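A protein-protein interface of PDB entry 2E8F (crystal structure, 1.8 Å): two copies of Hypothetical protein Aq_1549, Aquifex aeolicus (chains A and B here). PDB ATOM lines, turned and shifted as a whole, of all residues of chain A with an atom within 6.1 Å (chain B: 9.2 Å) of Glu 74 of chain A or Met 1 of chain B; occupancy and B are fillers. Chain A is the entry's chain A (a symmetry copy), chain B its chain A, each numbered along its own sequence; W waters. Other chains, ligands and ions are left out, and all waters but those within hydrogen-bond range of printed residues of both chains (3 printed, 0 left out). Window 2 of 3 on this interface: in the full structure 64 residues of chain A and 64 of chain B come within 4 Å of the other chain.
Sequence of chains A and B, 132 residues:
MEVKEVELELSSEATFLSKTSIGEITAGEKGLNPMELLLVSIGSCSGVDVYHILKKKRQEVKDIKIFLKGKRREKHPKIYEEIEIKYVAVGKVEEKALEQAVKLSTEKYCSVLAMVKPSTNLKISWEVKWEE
Among the printed residues, merely in contact across the chains: Lys 71 of chain A with Glu 2 of chain B, Arg 72 of chain A with Met 1 of chain B, Arg 72 of chain A with Lys 4 of chain B, His 76 of chain A with Lys 108 of chain B and Glu 81 of chain A with Met 1 of chain B.
Printed residues of chain B within 4 Å of Arg 72 of chain A: Met 1, Glu 2, Lys 4 and Ser 111.
Of chain B, only Met 1 (2.9 Å) comes within 4 Å of Glu 74 of chain A.
Lys 75 of chain A touches none of the printed residues of chain B.
Printed residues of chain B within 4 Å of Lys 78 of chain A: Ser 111.
Glu 82 of chain A touches none of the printed residues of chain B.
Met 1 of chain B touches just these residues of chain A: Arg 72, Glu 74 and Glu 81.
The nearest residue of chain B that does not touch Glu 74 of chain A is Glu 2 of chain B (5.5 Å).
The nearest residue of chain A that does not touch Met 1 of chain B is Lys 71 of chain A (4.03 Å).
The backbone NH (N) of Met 1 of chain B is in hydrogen-bond range of the side-chain carboxylate (OE2) of Glu 74 of chain A, at 2.9 Å.
NH1 of Arg 72 of chain A is in salt-bridge range of OE1 of Glu 2 of chain B.
The side-chain hydroxyl of Ser 111 of chain B is in hydrogen-bond range of the guanidinium group of Arg 72 of chain A (3.1 Å).
The side-chain hydroxyl (OG) of Ser 111 of chain B lies within hydrogen-bond range of the backbone NH (N) of Lys 78 of chain A (3.1 Å).
Water W3 lies within hydrogen-bond range of the backbone NH of Lys 78 of chain A and the side-chain hydroxyl of Ser 111 of chain B.
Water W2 lies within hydrogen-bond range of O of Arg 73 of chain A (3.0 Å), N of Glu 2 of chain B (3.1 Å) and O of Arg 72 of chain A (3.5 Å).
Water W1 bridges NH1 of Arg 72 of chain A (3.0 Å) and NZ of Lys 4 of chain B (3.3 Å).
The side-chain carboxylate of Glu 2 of chain B lies within salt-bridge range of the side-chain amino group of Lys 4 of chain B (3.0 Å).
The backbone carbonyl oxygen (O) of Lys 71 of chain A is in hydrogen-bond range of the backbone NH (N) of Glu 81 of chain A, 2.7 Å away.
The side-chain carboxylate of Glu 82 of chain A is in salt-bridge range of the side-chain amino group of Lys 71 of chain A (3.2 Å).
The guanidinium group (NE) of Arg 72 of chain A sits at hydrogen-bond distance from the backbone carbonyl oxygen (O) of Lys 78 of chain A, 2.9 Å away.
O of His 76 of chain A sits at hydrogen-bond distance from NH1 of Arg 73 of chain A, 3.1 Å away.
No position is printed for both chains.
Of the 9 printed residues of chain A, 6 touch a printed residue of chain B.
Hydrophobic or aromatic side chains of chain B within 4 Å of the printed part of chain A: Met 1.
Among the printed residues, 9 pairs touch across the chains.
Among the printed residues, Asp or Glu carboxylates within 4 Å of a Lys or Arg side-chain nitrogen of the other chain: Arg 72 of chain A with Glu 2 of chain B.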
ATOM      1  N   LYS A  71     -15.039  34.158  28.440  1.00  0.00           N
ATOM      2  CA  LYS A  71     -15.813  33.384  29.406  1.00  0.00           C
ATOM      3  C   LYS A  71     -16.944  32.711  28.636  1.00  0.00           C
ATOM      4  O   LYS A  71     -17.756  33.383  27.992  1.00  0.00           O
ATOM      5  CB  LYS A  71     -16.371  34.300  30.497  1.00  0.00           C
ATOM      6  CG  LYS A  71     -15.296  34.937  31.355  1.00  0.00           C
ATOM      7  CD  LYS A  71     -15.900  35.859  32.407  1.00  0.00           C
ATOM      8  CE  LYS A  71     -14.828  36.448  33.310  1.00  0.00           C
ATOM      9  NZ  LYS A  71     -13.820  37.244  32.551  1.00  0.00           N
ATOM     10  N   ARG A  72     -16.994  31.385  28.714  1.00  0.00           N
ATOM     11  CA  ARG A  72     -17.979  30.594  27.983  1.00  0.00           C
ATOM     12  C   ARG A  72     -19.271  30.265  28.718  1.00  0.00           C
ATOM     13  O   ARG A  72     -19.283  30.086  29.933  1.00  0.00           O
ATOM     14  CB  ARG A  72     -17.339  29.280  27.527  1.00  0.00           C
ATOM     15  CG  ARG A  72     -16.024  29.453  26.783  1.00  0.00           C
ATOM     16  CD  ARG A  72     -15.413  28.112  26.427  1.00  0.00           C
ATOM     17  NE  ARG A  72     -16.220  27.356  25.475  1.00  0.00           N
ATOM     18  CZ  ARG A  72     -15.878  26.162  25.001  1.00  0.00           C
ATOM     19  NH1 ARG A  72     -14.748  25.591  25.399  1.00  0.00           N
ATOM     20  NH2 ARG A  72     -16.643  25.551  24.110  1.00  0.00           N
ATOM     21  N   ARG A  73     -20.354  30.182  27.949  1.00  0.00           N
ATOM     22  CA  ARG A  73     -21.665  29.831  28.471  1.00  0.00           C
ATOM     23  C   ARG A  73     -21.530  28.379  28.913  1.00  0.00           C
ATOM     24  O   ARG A  73     -20.706  27.637  28.378  1.00  0.00           O
ATOM     25  CB  ARG A  73     -22.720  29.928  27.365  1.00  0.00           C
ATOM     26  CG  ARG A  73     -24.146  29.909  27.866  1.00  0.00           C
ATOM     27  CD  ARG A  73     -25.045  29.089  26.965  1.00  0.00           C
ATOM     28  NE  ARG A  73     -24.950  29.456  25.556  1.00  0.00           N
ATOM     29  CZ  ARG A  73     -25.617  28.839  24.587  1.00  0.00           C
ATOM     30  NH1 ARG A  73     -26.426  27.827  24.880  1.00  0.00           N
ATOM     31  NH2 ARG A  73     -25.479  29.221  23.327  1.00  0.00           N
ATOM     32  N   GLU A  74     -22.349  27.964  29.870  1.00  0.00           N
ATOM     33  CA  GLU A  74     -22.263  26.603  30.368  1.00  0.00           C
ATOM     34  C   GLU A  74     -23.011  25.565  29.538  1.00  0.00           C
ATOM     35  O   GLU A  74     -22.624  24.400  29.522  1.00  0.00           O
ATOM     36  CB  GLU A  74     -22.697  26.583  31.837  1.00  0.00           C
ATOM     37  CG  GLU A  74     -21.706  27.356  32.701  1.00  0.00           C
ATOM     38  CD  GLU A  74     -22.199  27.648  34.103  1.00  0.00           C
ATOM     39  OE1 GLU A  74     -23.311  27.204  34.460  1.00  0.00           O
ATOM     40  OE2 GLU A  74     -21.463  28.334  34.849  1.00  0.00           O
ATOM     41  N   LYS A  75     -24.066  25.967  28.835  1.00  0.00           N
ATOM     42  CA  LYS A  75     -24.780  25.002  28.012  1.00  0.00           C
ATOM     43  C   LYS A  75     -24.415  25.163  26.537  1.00  0.00           C
ATOM     44  O   LYS A  75     -23.926  26.213  26.119  1.00  0.00           O
ATOM     45  CB  LYS A  75     -26.293  25.114  28.205  1.00  0.00           C
ATOM     46  CG  LYS A  75     -26.946  26.375  27.685  1.00  0.00           C
ATOM     47  CD  LYS A  75     -28.463  26.192  27.686  1.00  0.00           C
ATOM     48  CE  LYS A  75     -29.194  27.474  27.336  1.00  0.00           C
ATOM     49  NZ  LYS A  75     -28.795  28.015  26.006  1.00  0.00           N
ATOM     50  N   HIS A  76     -24.643  24.111  25.754  1.00  0.00           N
ATOM     51  CA  HIS A  76     -24.307  24.129  24.333  1.00  0.00           C
ATOM     52  C   HIS A  76     -25.246  24.958  23.467  1.00  0.00           C
ATOM     53  O   HIS A  76     -26.462  24.946  23.661  1.00  0.00           O
ATOM     54  CB  HIS A  76     -24.252  22.701  23.784  1.00  0.00           C
ATOM     55  CG  HIS A  76     -23.275  21.815  24.493  1.00  0.00           C
ATOM     56  ND1 HIS A  76     -23.654  20.925  25.476  1.00  0.00           N
ATOM     57  CD2 HIS A  76     -21.933  21.683  24.364  1.00  0.00           C
ATOM     58  CE1 HIS A  76     -22.588  20.282  25.919  1.00  0.00           C
ATOM     59  NE2 HIS A  76     -21.532  20.722  25.260  1.00  0.00           N
ATOM     60  N   LYS A  78     -21.384  26.279  23.738  1.00  0.00           N
ATOM     61  CA  LYS A  78     -20.634  27.025  24.731  1.00  0.00           C
ATOM     62  C   LYS A  78     -19.864  28.219  24.176  1.00  0.00           C
ATOM     63  O   LYS A  78     -18.643  28.286  24.292  1.00  0.00           O
ATOM     64  CB  LYS A  78     -19.694  26.058  25.452  1.00  0.00           C
ATOM     65  CG  LYS A  78     -20.454  25.028  26.297  1.00  0.00           C
ATOM     66  CD  LYS A  78     -19.530  24.005  26.956  1.00  0.00           C
ATOM     67  CE  LYS A  78     -20.152  23.506  28.249  1.00  0.00           C
ATOM     68  NZ  LYS A  78     -19.771  22.095  28.537  1.00  0.00           N
ATOM     69  N   GLU A  81     -19.653  34.285  26.229  1.00  0.00           N
ATOM     70  CA  GLU A  81     -20.692  35.250  26.573  1.00  0.00           C
ATOM     71  C   GLU A  81     -19.998  36.588  26.752  1.00  0.00           C
ATOM     72  O   GLU A  81     -20.620  37.648  26.667  1.00  0.00           O
ATOM     73  CB  GLU A  81     -21.390  34.867  27.882  1.00  0.00           C
ATOM     74  CG  GLU A  81     -22.059  33.502  27.859  1.00  0.00           C
ATOM     75  CD  GLU A  81     -23.379  33.474  28.611  1.00  0.00           C
ATOM     76  OE1 GLU A  81     -23.398  33.795  29.819  1.00  0.00           O
ATOM     77  OE2 GLU A  81     -24.404  33.132  27.984  1.00  0.00           O
ATOM     78  N   GLU A  82     -18.693  36.524  26.981  1.00  0.00           N
ATOM     79  CA  GLU A  82     -17.897  37.720  27.197  1.00  0.00           C
ATOM     80  C   GLU A  82     -16.476  37.532  26.685  1.00  0.00           C
ATOM     81  O   GLU A  82     -15.901  36.450  26.783  1.00  0.00           O
ATOM     82  CB  GLU A  82     -17.869  38.048  28.698  1.00  0.00           C
ATOM     83  CG  GLU A  82     -16.942  39.185  29.102  1.00  0.00           C
ATOM     84  CD  GLU A  82     -16.848  39.342  30.618  1.00  0.00           C
ATOM     85  OE1 GLU A  82     -17.902  39.376  31.288  1.00  0.00           O
ATOM     86  OE2 GLU A  82     -15.720  39.439  31.136  1.00  0.00           O
ATOM     87  N   MET B   1     -18.679  28.931  34.246  1.00  0.00           N
ATOM     88  CA  MET B   1     -18.225  29.513  32.953  1.00  0.00           C
ATOM     89  C   MET B   1     -16.738  29.264  32.733  1.00  0.00           C
ATOM     90  O   MET B   1     -15.893  29.815  33.440  1.00  0.00           O
ATOM     91  CB  MET B   1     -18.509  31.018  32.928  1.00  0.00           C
ATOM     92  CG  MET B   1     -19.987  31.369  33.016  1.00  0.00           C
ATOM     93  SD  MET B   1     -20.301  33.131  32.783  1.00  0.00           S
ATOM     94  CE  MET B   1     -20.405  33.209  31.023  1.00  0.00           C
ATOM     95  N   GLU B   2     -16.415  28.429  31.753  1.00  0.00           N
ATOM     96  CA  GLU B   2     -15.017  28.146  31.482  1.00  0.00           C
ATOM     97  C   GLU B   2     -14.344  29.388  30.929  1.00  0.00           C
ATOM     98  O   GLU B   2     -14.929  30.140  30.145  1.00  0.00           O
ATOM     99  CB  GLU B   2     -14.843  26.993  30.486  1.00  0.00           C
ATOM    100  CG  GLU B   2     -13.381  26.788  30.092  1.00  0.00           C
ATOM    101  CD  GLU B   2     -13.154  25.639  29.123  1.00  0.00           C
ATOM    102  OE1 GLU B   2     -13.986  25.448  28.215  1.00  0.00           O
ATOM    103  OE2 GLU B   2     -12.127  24.938  29.265  1.00  0.00           O
ATOM    104  N   VAL B   3     -13.106  29.599  31.349  1.00  0.00           N
ATOM    105  CA  VAL B   3     -12.341  30.739  30.894  1.00  0.00           C
ATOM    106  C   VAL B   3     -11.233  30.268  29.962  1.00  0.00           C
ATOM    107  O   VAL B   3     -10.556  29.275  30.240  1.00  0.00           O
ATOM    108  CB  VAL B   3     -11.694  31.481  32.085  1.00  0.00           C
ATOM    109  CG1 VAL B   3     -10.879  32.665  31.581  1.00  0.00           C
ATOM    110  CG2 VAL B   3     -12.762  31.945  33.045  1.00  0.00           C
ATOM    111  N   LYS B   4     -11.073  30.965  28.843  1.00  0.00           N
ATOM    112  CA  LYS B   4     -10.014  30.664  27.887  1.00  0.00           C
ATOM    113  C   LYS B   4      -9.194  31.946  27.798  1.00  0.00           C
ATOM    114  O   LYS B   4      -9.762  33.037  27.762  1.00  0.00           O
ATOM    115  CB  LYS B   4     -10.584  30.334  26.504  1.00  0.00           C
ATOM    116  CG  LYS B   4     -11.358  29.028  26.410  1.00  0.00           C
ATOM    117  CD  LYS B   4     -10.476  27.813  26.653  1.00  0.00           C
ATOM    118  CE  LYS B   4     -11.202  26.539  26.235  1.00  0.00           C
ATOM    119  NZ  LYS B   4     -10.542  25.303  26.725  1.00  0.00           N
ATOM    120  N   LYS B 108     -25.909  22.671  17.228  1.00  0.00           N
ATOM    121  CA  LYS B 108     -25.918  22.607  18.686  1.00  0.00           C
ATOM    122  C   LYS B 108     -24.584  22.658  19.430  1.00  0.00           C
ATOM    123  O   LYS B 108     -24.444  23.394  20.404  1.00  0.00           O
ATOM    124  CB  LYS B 108     -26.675  21.356  19.143  1.00  0.00           C
ATOM    125  CG  LYS B 108     -26.643  21.132  20.645  1.00  0.00           C
ATOM    126  CD  LYS B 108     -27.420  19.883  21.042  1.00  0.00           C
ATOM    127  CE  LYS B 108     -27.469  19.721  22.554  1.00  0.00           C
ATOM    128  NZ  LYS B 108     -28.154  20.877  23.202  1.00  0.00           N
ATOM    129  N   SER B 111     -19.155  25.659  19.144  1.00  0.00           N
ATOM    130  CA  SER B 111     -19.110  26.990  19.748  1.00  0.00           C
ATOM    131  C   SER B 111     -18.588  28.089  18.823  1.00  0.00           C
ATOM    132  O   SER B 111     -19.157  29.181  18.770  1.00  0.00           O
ATOM    133  CB  SER B 111     -18.250  26.967  21.020  1.00  0.00           C
ATOM    134  OG  SER B 111     -18.828  26.160  22.036  1.00  0.00           O
HETATM  135  O   HOH W   1     -12.613  23.519  24.866  1.00  0.00           O
HETATM  136  O   HOH W   2     -18.333  26.752  29.933  1.00  0.00           O
HETATM  137  O   HOH W   3     -20.435  23.653  22.909  1.00  0.00           O
